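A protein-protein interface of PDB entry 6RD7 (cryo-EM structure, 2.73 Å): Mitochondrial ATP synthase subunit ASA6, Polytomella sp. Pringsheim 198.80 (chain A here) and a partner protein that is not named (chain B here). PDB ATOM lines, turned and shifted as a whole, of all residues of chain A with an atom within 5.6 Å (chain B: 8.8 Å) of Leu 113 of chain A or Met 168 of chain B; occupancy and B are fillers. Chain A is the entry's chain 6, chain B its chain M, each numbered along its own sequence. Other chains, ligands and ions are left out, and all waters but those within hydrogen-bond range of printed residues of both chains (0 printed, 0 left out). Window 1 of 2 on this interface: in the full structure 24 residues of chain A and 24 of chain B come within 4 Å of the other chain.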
ATOM      1  N   GLN A 109      19.250  12.040   9.491  1.00  0.00           N
ATOM      2  CA  GLN A 109      17.945  12.647   9.245  1.00  0.00           C
ATOM      3  C   GLN A 109      17.731  13.895  10.102  1.00  0.00           C
ATOM      4  O   GLN A 109      17.152  14.892   9.634  1.00  0.00           O
ATOM      5  CB  GLN A 109      16.851  11.612   9.485  1.00  0.00           C
ATOM      6  CG  GLN A 109      16.865  10.498   8.455  1.00  0.00           C
ATOM      7  CD  GLN A 109      16.245   9.221   8.961  1.00  0.00           C
ATOM      8  OE1 GLN A 109      16.094   9.027  10.161  1.00  0.00           O
ATOM      9  NE2 GLN A 109      15.888   8.335   8.044  1.00  0.00           N
ATOM     10  N   ALA A 110      18.200  13.868  11.354  1.00  0.00           N
ATOM     11  CA  ALA A 110      18.112  15.046  12.208  1.00  0.00           C
ATOM     12  C   ALA A 110      18.963  16.197  11.695  1.00  0.00           C
ATOM     13  O   ALA A 110      18.598  17.361  11.905  1.00  0.00           O
ATOM     14  CB  ALA A 110      18.523  14.693  13.634  1.00  0.00           C
ATOM     15  N   ALA A 111      20.065  15.892  11.003  1.00  0.00           N
ATOM     16  CA  ALA A 111      20.870  16.927  10.366  1.00  0.00           C
ATOM     17  C   ALA A 111      20.091  17.684   9.303  1.00  0.00           C
ATOM     18  O   ALA A 111      20.180  18.912   9.233  1.00  0.00           O
ATOM     19  CB  ALA A 111      22.113  16.310   9.742  1.00  0.00           C
ATOM     20  N   TRP A 112      19.312  16.984   8.485  1.00  0.00           N
ATOM     21  CA  TRP A 112      18.535  17.675   7.468  1.00  0.00           C
ATOM     22  C   TRP A 112      17.328  18.389   8.042  1.00  0.00           C
ATOM     23  O   TRP A 112      16.911  19.403   7.480  1.00  0.00           O
ATOM     24  CB  TRP A 112      18.090  16.715   6.371  1.00  0.00           C
ATOM     25  CG  TRP A 112      18.994  16.742   5.194  1.00  0.00           C
ATOM     26  CD1 TRP A 112      19.825  15.751   4.796  1.00  0.00           C
ATOM     27  CD2 TRP A 112      19.192  17.821   4.265  1.00  0.00           C
ATOM     28  NE1 TRP A 112      20.518  16.123   3.676  1.00  0.00           N
ATOM     29  CE2 TRP A 112      20.147  17.392   3.330  1.00  0.00           C
ATOM     30  CE3 TRP A 112      18.654  19.101   4.139  1.00  0.00           C
ATOM     31  CZ2 TRP A 112      20.573  18.191   2.282  1.00  0.00           C
ATOM     32  CZ3 TRP A 112      19.067  19.898   3.102  1.00  0.00           C
ATOM     33  CH2 TRP A 112      20.024  19.441   2.181  1.00  0.00           C
ATOM     34  N   LEU A 113      16.775  17.902   9.158  1.00  0.00           N
ATOM     35  CA  LEU A 113      15.763  18.689   9.869  1.00  0.00           C
ATOM     36  C   LEU A 113      16.339  20.014  10.369  1.00  0.00           C
ATOM     37  O   LEU A 113      15.720  21.080  10.210  1.00  0.00           O
ATOM     38  CB  LEU A 113      15.197  17.883  11.034  1.00  0.00           C
ATOM     39  CG  LEU A 113      13.856  17.180  10.853  1.00  0.00           C
ATOM     40  CD1 LEU A 113      13.959  16.070   9.842  1.00  0.00           C
ATOM     41  CD2 LEU A 113      13.387  16.636  12.182  1.00  0.00           C
ATOM     42  N   ILE A 114      17.545  19.963  10.939  1.00  0.00           N
ATOM     43  CA  ILE A 114      18.222  21.165  11.419  1.00  0.00           C
ATOM     44  C   ILE A 114      18.551  22.105  10.260  1.00  0.00           C
ATOM     45  O   ILE A 114      18.395  23.327  10.372  1.00  0.00           O
ATOM     46  CB  ILE A 114      19.471  20.751  12.222  1.00  0.00           C
ATOM     47  CG1 ILE A 114      19.053  20.195  13.582  1.00  0.00           C
ATOM     48  CG2 ILE A 114      20.425  21.901  12.424  1.00  0.00           C
ATOM     49  CD1 ILE A 114      20.153  19.459  14.293  1.00  0.00           C
ATOM     50  N   SER A 115      18.952  21.552   9.113  1.00  0.00           N
ATOM     51  CA  SER A 115      19.252  22.389   7.953  1.00  0.00           C
ATOM     52  C   SER A 115      17.994  22.978   7.323  1.00  0.00           C
ATOM     53  O   SER A 115      18.050  24.062   6.738  1.00  0.00           O
ATOM     54  CB  SER A 115      20.025  21.589   6.914  1.00  0.00           C
ATOM     55  OG  SER A 115      21.293  21.206   7.414  1.00  0.00           O
ATOM     56  N   PHE A 116      16.861  22.277   7.415  1.00  0.00           N
ATOM     57  CA  PHE A 116      15.582  22.837   6.983  1.00  0.00           C
ATOM     58  C   PHE A 116      15.164  24.002   7.854  1.00  0.00           C
ATOM     59  O   PHE A 116      14.520  24.938   7.374  1.00  0.00           O
ATOM     60  CB  PHE A 116      14.498  21.772   7.025  1.00  0.00           C
ATOM     61  CG  PHE A 116      14.546  20.818   5.890  1.00  0.00           C
ATOM     62  CD1 PHE A 116      15.124  21.174   4.682  1.00  0.00           C
ATOM     63  CD2 PHE A 116      14.050  19.545   6.040  1.00  0.00           C
ATOM     64  CE1 PHE A 116      15.164  20.275   3.634  1.00  0.00           C
ATOM     65  CE2 PHE A 116      14.106  18.655   5.006  1.00  0.00           C
ATOM     66  CZ  PHE A 116      14.661  19.008   3.800  1.00  0.00           C
ATOM     67  N   SER A 117      15.491  23.943   9.145  1.00  0.00           N
ATOM     68  CA  SER A 117      15.194  25.066  10.030  1.00  0.00           C
ATOM     69  C   SER A 117      16.006  26.305   9.655  1.00  0.00           C
ATOM     70  O   SER A 117      15.592  27.437   9.922  1.00  0.00           O
ATOM     71  CB  SER A 117      15.460  24.665  11.475  1.00  0.00           C
ATOM     72  OG  SER A 117      14.516  23.701  11.901  1.00  0.00           O
ATOM     73  N   SER A 118      17.160  26.105   9.019  1.00  0.00           N
ATOM     74  CA  SER A 118      18.043  27.218   8.696  1.00  0.00           C
ATOM     75  C   SER A 118      17.773  27.758   7.297  1.00  0.00           C
ATOM     76  O   SER A 118      17.845  28.970   7.064  1.00  0.00           O
ATOM     77  CB  SER A 118      19.497  26.764   8.819  1.00  0.00           C
ATOM     78  OG  SER A 118      19.856  26.561  10.171  1.00  0.00           O
ATOM     79  N   ILE B 160       2.602  11.166   0.516  1.00  0.00           N
ATOM     80  CA  ILE B 160       3.644  12.109   0.907  1.00  0.00           C
ATOM     81  C   ILE B 160       3.853  12.077   2.419  1.00  0.00           C
ATOM     82  O   ILE B 160       4.976  12.264   2.897  1.00  0.00           O
ATOM     83  CB  ILE B 160       3.347  13.526   0.371  1.00  0.00           C
ATOM     84  CG1 ILE B 160       4.652  14.312   0.250  1.00  0.00           C
ATOM     85  CG2 ILE B 160       2.358  14.295   1.231  1.00  0.00           C
ATOM     86  CD1 ILE B 160       4.519  15.596  -0.506  1.00  0.00           C
ATOM     87  N   SER B 161       2.816  11.710   3.183  1.00  0.00           N
ATOM     88  CA  SER B 161       2.994  11.551   4.622  1.00  0.00           C
ATOM     89  C   SER B 161       3.825  10.316   4.943  1.00  0.00           C
ATOM     90  O   SER B 161       4.761  10.379   5.749  1.00  0.00           O
ATOM     91  CB  SER B 161       1.634  11.478   5.305  1.00  0.00           C
ATOM     92  OG  SER B 161       1.056  12.763   5.403  1.00  0.00           O
ATOM     93  N   CYS B 162       3.520   9.193   4.294  1.00  0.00           N
ATOM     94  CA  CYS B 162       4.261   7.961   4.534  1.00  0.00           C
ATOM     95  C   CYS B 162       5.673   8.041   3.966  1.00  0.00           C
ATOM     96  O   CYS B 162       6.587   7.382   4.467  1.00  0.00           O
ATOM     97  CB  CYS B 162       3.506   6.774   3.943  1.00  0.00           C
ATOM     98  SG  CYS B 162       1.981   6.358   4.797  1.00  0.00           S
ATOM     99  N   ASN B 163       5.873   8.848   2.926  1.00  0.00           N
ATOM    100  CA  ASN B 163       7.207   9.011   2.365  1.00  0.00           C
ATOM    101  C   ASN B 163       8.061   9.912   3.240  1.00  0.00           C
ATOM    102  O   ASN B 163       9.252   9.652   3.428  1.00  0.00           O
ATOM    103  CB  ASN B 163       7.120   9.576   0.949  1.00  0.00           C
ATOM    104  CG  ASN B 163       6.756   8.535  -0.078  1.00  0.00           C
ATOM    105  OD1 ASN B 163       6.587   8.841  -1.253  1.00  0.00           O
ATOM    106  ND2 ASN B 163       6.613   7.302   0.362  1.00  0.00           N
ATOM    107  N   LEU B 164       7.472  10.977   3.790  1.00  0.00           N
ATOM    108  CA  LEU B 164       8.231  11.841   4.680  1.00  0.00           C
ATOM    109  C   LEU B 164       8.381  11.246   6.071  1.00  0.00           C
ATOM    110  O   LEU B 164       9.170  11.765   6.865  1.00  0.00           O
ATOM    111  CB  LEU B 164       7.574  13.216   4.764  1.00  0.00           C
ATOM    112  CG  LEU B 164       7.653  14.080   3.506  1.00  0.00           C
ATOM    113  CD1 LEU B 164       6.947  15.398   3.735  1.00  0.00           C
ATOM    114  CD2 LEU B 164       9.087  14.305   3.084  1.00  0.00           C
ATOM    115  N   LEU B 165       7.631  10.188   6.393  1.00  0.00           N
ATOM    116  CA  LEU B 165       7.883   9.460   7.633  1.00  0.00           C
ATOM    117  C   LEU B 165       9.242   8.774   7.611  1.00  0.00           C
ATOM    118  O   LEU B 165       9.885   8.629   8.654  1.00  0.00           O
ATOM    119  CB  LEU B 165       6.786   8.431   7.879  1.00  0.00           C
ATOM    120  CG  LEU B 165       5.592   8.880   8.709  1.00  0.00           C
ATOM    121  CD1 LEU B 165       4.627   7.729   8.889  1.00  0.00           C
ATOM    122  CD2 LEU B 165       6.061   9.404  10.046  1.00  0.00           C
ATOM    123  N   GLY B 166       9.699   8.352   6.434  1.00  0.00           N
ATOM    124  CA  GLY B 166      10.969   7.650   6.353  1.00  0.00           C
ATOM    125  C   GLY B 166      12.162   8.564   6.539  1.00  0.00           C
ATOM    126  O   GLY B 166      13.267   8.105   6.833  1.00  0.00           O
ATOM    127  N   LEU B 167      11.957   9.863   6.370  1.00  0.00           N
ATOM    128  CA  LEU B 167      13.011  10.847   6.549  1.00  0.00           C
ATOM    129  C   LEU B 167      12.998  11.486   7.929  1.00  0.00           C
ATOM    130  O   LEU B 167      13.843  12.341   8.204  1.00  0.00           O
ATOM    131  CB  LEU B 167      12.890  11.918   5.475  1.00  0.00           C
ATOM    132  CG  LEU B 167      13.042  11.328   4.081  1.00  0.00           C
ATOM    133  CD1 LEU B 167      12.132  12.024   3.105  1.00  0.00           C
ATOM    134  CD2 LEU B 167      14.479  11.445   3.656  1.00  0.00           C
ATOM    135  N   MET B 168      12.063  11.107   8.786  1.00  0.00           N
ATOM    136  CA  MET B 168      12.115  11.577  10.159  1.00  0.00           C
ATOM    137  C   MET B 168      13.023  10.667  10.978  1.00  0.00           C
ATOM    138  O   MET B 168      13.116   9.473  10.687  1.00  0.00           O
ATOM    139  CB  MET B 168      10.719  11.602  10.774  1.00  0.00           C
ATOM    140  CG  MET B 168       9.788  12.605  10.127  1.00  0.00           C
ATOM    141  SD  MET B 168      10.523  14.245  10.011  1.00  0.00           S
ATOM    142  CE  MET B 168      10.260  14.619   8.283  1.00  0.00           C
ATOM    143  N   PRO B 169      13.728  11.212  11.970  1.00  0.00           N
ATOM    144  CA  PRO B 169      14.588  10.373  12.812  1.00  0.00           C
ATOM    145  C   PRO B 169      13.779   9.374  13.626  1.00  0.00           C
ATOM    146  O   PRO B 169      12.642   9.640  14.016  1.00  0.00           O
ATOM    147  CB  PRO B 169      15.308  11.386  13.709  1.00  0.00           C
ATOM    148  CG  PRO B 169      14.585  12.666  13.535  1.00  0.00           C
ATOM    149  CD  PRO B 169      13.987  12.642  12.182  1.00  0.00           C
ATOM    150  N   PHE B 170      14.373   8.192  13.818  1.00  0.00           N
ATOM    151  CA  PHE B 170      13.833   7.005  14.484  1.00  0.00           C
ATOM    152  C   PHE B 170      12.632   6.393  13.776  1.00  0.00           C
ATOM    153  O   PHE B 170      12.019   5.475  14.315  1.00  0.00           O
ATOM    154  CB  PHE B 170      13.461   7.264  15.952  1.00  0.00           C
ATOM    155  CG  PHE B 170      14.562   7.875  16.760  1.00  0.00           C
ATOM    156  CD1 PHE B 170      15.552   7.083  17.308  1.00  0.00           C
ATOM    157  CD2 PHE B 170      14.603   9.240  16.979  1.00  0.00           C
ATOM    158  CE1 PHE B 170      16.565   7.638  18.051  1.00  0.00           C
ATOM    159  CE2 PHE B 170      15.616   9.802  17.721  1.00  0.00           C
ATOM    160  CZ  PHE B 170      16.597   8.999  18.258  1.00  0.00           C
ATOM    161  N   ASN B 171      12.287   6.841  12.577  1.00  0.00           N
ATOM    162  CA  ASN B 171      11.092   6.365  11.904  1.00  0.00           C
ATOM    163  C   ASN B 171      11.452   5.763  10.557  1.00  0.00           C
ATOM    164  O   ASN B 171      12.461   6.124   9.946  1.00  0.00           O
ATOM    165  CB  ASN B 171      10.082   7.492  11.715  1.00  0.00           C
ATOM    166  CG  ASN B 171       9.277   7.764  12.960  1.00  0.00           C
ATOM    167  OD1 ASN B 171       8.440   6.961  13.356  1.00  0.00           O
ATOM    168  ND2 ASN B 171       9.531   8.903  13.589  1.00  0.00           N
ATOM    169  N   GLU B 172      10.619   4.836  10.104  1.00  0.00           N
ATOM    170  CA  GLU B 172      10.748   4.234   8.789  1.00  0.00           C
ATOM    171  C   GLU B 172       9.509   4.566   7.976  1.00  0.00           C
ATOM    172  O   GLU B 172       8.453   4.877   8.533  1.00  0.00           O
ATOM    173  CB  GLU B 172      10.934   2.714   8.875  1.00  0.00           C
ATOM    174  CG  GLU B 172       9.696   1.948   9.307  1.00  0.00           C
ATOM    175  CD  GLU B 172      10.000   0.519   9.711  1.00  0.00           C
ATOM    176  OE1 GLU B 172      11.176   0.112   9.617  1.00  0.00           O
ATOM    177  OE2 GLU B 172       9.065  -0.196  10.127  1.00  0.00           O
ATOM    178  N   ALA B 173       9.649   4.522   6.662  1.00  0.00           N
ATOM    179  CA  ALA B 173       8.509   4.761   5.801  1.00  0.00           C
ATOM    180  C   ALA B 173       7.622   3.521   5.764  1.00  0.00           C
ATOM    181  O   ALA B 173       8.126   2.406   5.604  1.00  0.00           O
ATOM    182  CB  ALA B 173       8.972   5.114   4.391  1.00  0.00           C
ATOM    183  N   HIS B 248      17.139   4.553   0.872  1.00  0.00           N
ATOM    184  CA  HIS B 248      17.288   4.007   2.208  1.00  0.00           C
ATOM    185  C   HIS B 248      18.325   2.892   2.259  1.00  0.00           C
ATOM    186  O   HIS B 248      19.194   2.901   3.138  1.00  0.00           O
ATOM    187  CB  HIS B 248      15.944   3.512   2.718  1.00  0.00           C
ATOM    188  CG  HIS B 248      15.896   3.414   4.199  1.00  0.00           C
ATOM    189  ND1 HIS B 248      16.320   4.440   5.010  1.00  0.00           N
ATOM    190  CD2 HIS B 248      15.527   2.406   5.022  1.00  0.00           C
ATOM    191  CE1 HIS B 248      16.189   4.080   6.272  1.00  0.00           C
ATOM    192  NE2 HIS B 248      15.711   2.851   6.307  1.00  0.00           N
ATOM    193  N   VAL B 285      20.612  12.018   1.502  1.00  0.00           N
ATOM    194  CA  VAL B 285      19.370  12.217   2.256  1.00  0.00           C
ATOM    195  C   VAL B 285      18.549  13.373   1.665  1.00  0.00           C
ATOM    196  O   VAL B 285      17.309  13.304   1.627  1.00  0.00           O
ATOM    197  CB  VAL B 285      19.652  12.426   3.756  1.00  0.00           C
ATOM    198  CG1 VAL B 285      18.361  12.488   4.555  1.00  0.00           C
ATOM    199  CG2 VAL B 285      20.481  11.314   4.304  1.00  0.00           C
ATOM    200  N   GLU B 288      16.856  11.947  -1.167  1.00  0.00           N
ATOM    201  CA  GLU B 288      15.741  11.139  -0.683  1.00  0.00           C
ATOM    202  C   GLU B 288      14.516  11.979  -0.370  1.00  0.00           C
ATOM    203  O   GLU B 288      13.389  11.524  -0.585  1.00  0.00           O
ATOM    204  CB  GLU B 288      16.154  10.376   0.562  1.00  0.00           C
ATOM    205  CG  GLU B 288      16.653   9.003   0.303  1.00  0.00           C
ATOM    206  CD  GLU B 288      16.556   8.149   1.532  1.00  0.00           C
ATOM    207  OE1 GLU B 288      15.424   7.866   1.975  1.00  0.00           O
ATOM    208  OE2 GLU B 288      17.614   7.804   2.084  1.00  0.00           O
ATOM    209  N   TYR B 289      14.718  13.193   0.146  1.00  0.00           N
ATOM    210  CA  TYR B 289      13.605  14.124   0.348  1.00  0.00           C
ATOM    211  C   TYR B 289      12.931  14.471  -0.973  1.00  0.00           C
ATOM    212  O   TYR B 289      11.688  14.450  -1.087  1.00  0.00           O
ATOM    213  CB  TYR B 289      14.107  15.397   1.025  1.00  0.00           C
ATOM    214  CG  TYR B 289      14.023  15.360   2.521  1.00  0.00           C
ATOM    215  CD1 TYR B 289      12.818  15.576   3.169  1.00  0.00           C
ATOM    216  CD2 TYR B 289      15.149  15.106   3.288  1.00  0.00           C
ATOM    217  CE1 TYR B 289      12.735  15.530   4.539  1.00  0.00           C
ATOM    218  CE2 TYR B 289      15.080  15.063   4.658  1.00  0.00           C
ATOM    219  CZ  TYR B 289      13.872  15.278   5.279  1.00  0.00           C
ATOM    220  OH  TYR B 289      13.800  15.238   6.646  1.00  0.00           O
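The backbone carbonyl oxygen (O) of Leu 167 of chain B is in hydrogen-bond range of the side-chain hydroxyl (OH) of Tyr 289 of chain B. The backbone carbonyl oxygen of Pro 169 of chain B is in hydrogen-bond range of the side-chain amide nitrogen of Asn 171 of chain B. The backbone carbonyl oxygen (O) of Leu 113 of chain A is in hydrogen-bond range of the side-chain hydroxyl (OG) of Ser 117 of chain A, 3.3 Å away.
Of the printed residues of chain B, Gln 109 of chain A touches Gly 166, Leu 167, Met 168 and Pro 169. Of the printed residues of chain B, Trp 112 of chain A touches Val 285 and Tyr 289. Ser 161 of chain B touches none of the printed residues of chain A. Leu 165 of chain B touches none of the printed residues of chain A. Met 168 of chain B touches two residues of chain A. The nearest residue of chain B that does not touch Leu 113 of chain A is Pro 169 of chain B (4.04 Å). The nearest printed residue of chain A that does not touch Leu 167 of chain B is Leu 113 of chain A (4.1 Å).
The side-chain amide nitrogen (NE2) of Gln 109 of chain A is in hydrogen-bond range of the backbone carbonyl oxygen (O) of Gly 166 of chain B (2.9 Å). The side-chain amide oxygen (OE1) of Gln 109 of chain A lies close to the backbone carbonyl oxygen (O) of Met 168 of chain B (3.1 Å).
Among the printed residues, pairs that only touch across the chains: Leu 113 of chain A with Tyr 289 of chain B, Gln 109 of chain A with Pro 169 of chain B, Gln 109 of chain A with Leu 167 of chain B, Phe 116 of chain A with Tyr 289 of chain B, Trp 112 of chain A with Val 285 of chain B, Trp 112 of chain A with Tyr 289 of chain B and Leu 113 of chain A with Met 168 of chain B.
Printed residues of chain B that touch a printed residue of chain A: Gly 166, Leu 167, Met 168, Pro 169, Val 285 and Tyr 289. Hydrophobic or aromatic side chains of chain B within 4 Å of the printed part of chain A: Met 168, Val 285 and Tyr 289. Along chain B the printed residues that touch a printed residue of chain A span positions 166 to 289. Among the printed residues, 9 pairs touch across the chains. Among the printed residues, no Asp or Glu carboxylate lies within 4 Å of a Lys or Arg side-chain nitrogen of the other chain.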
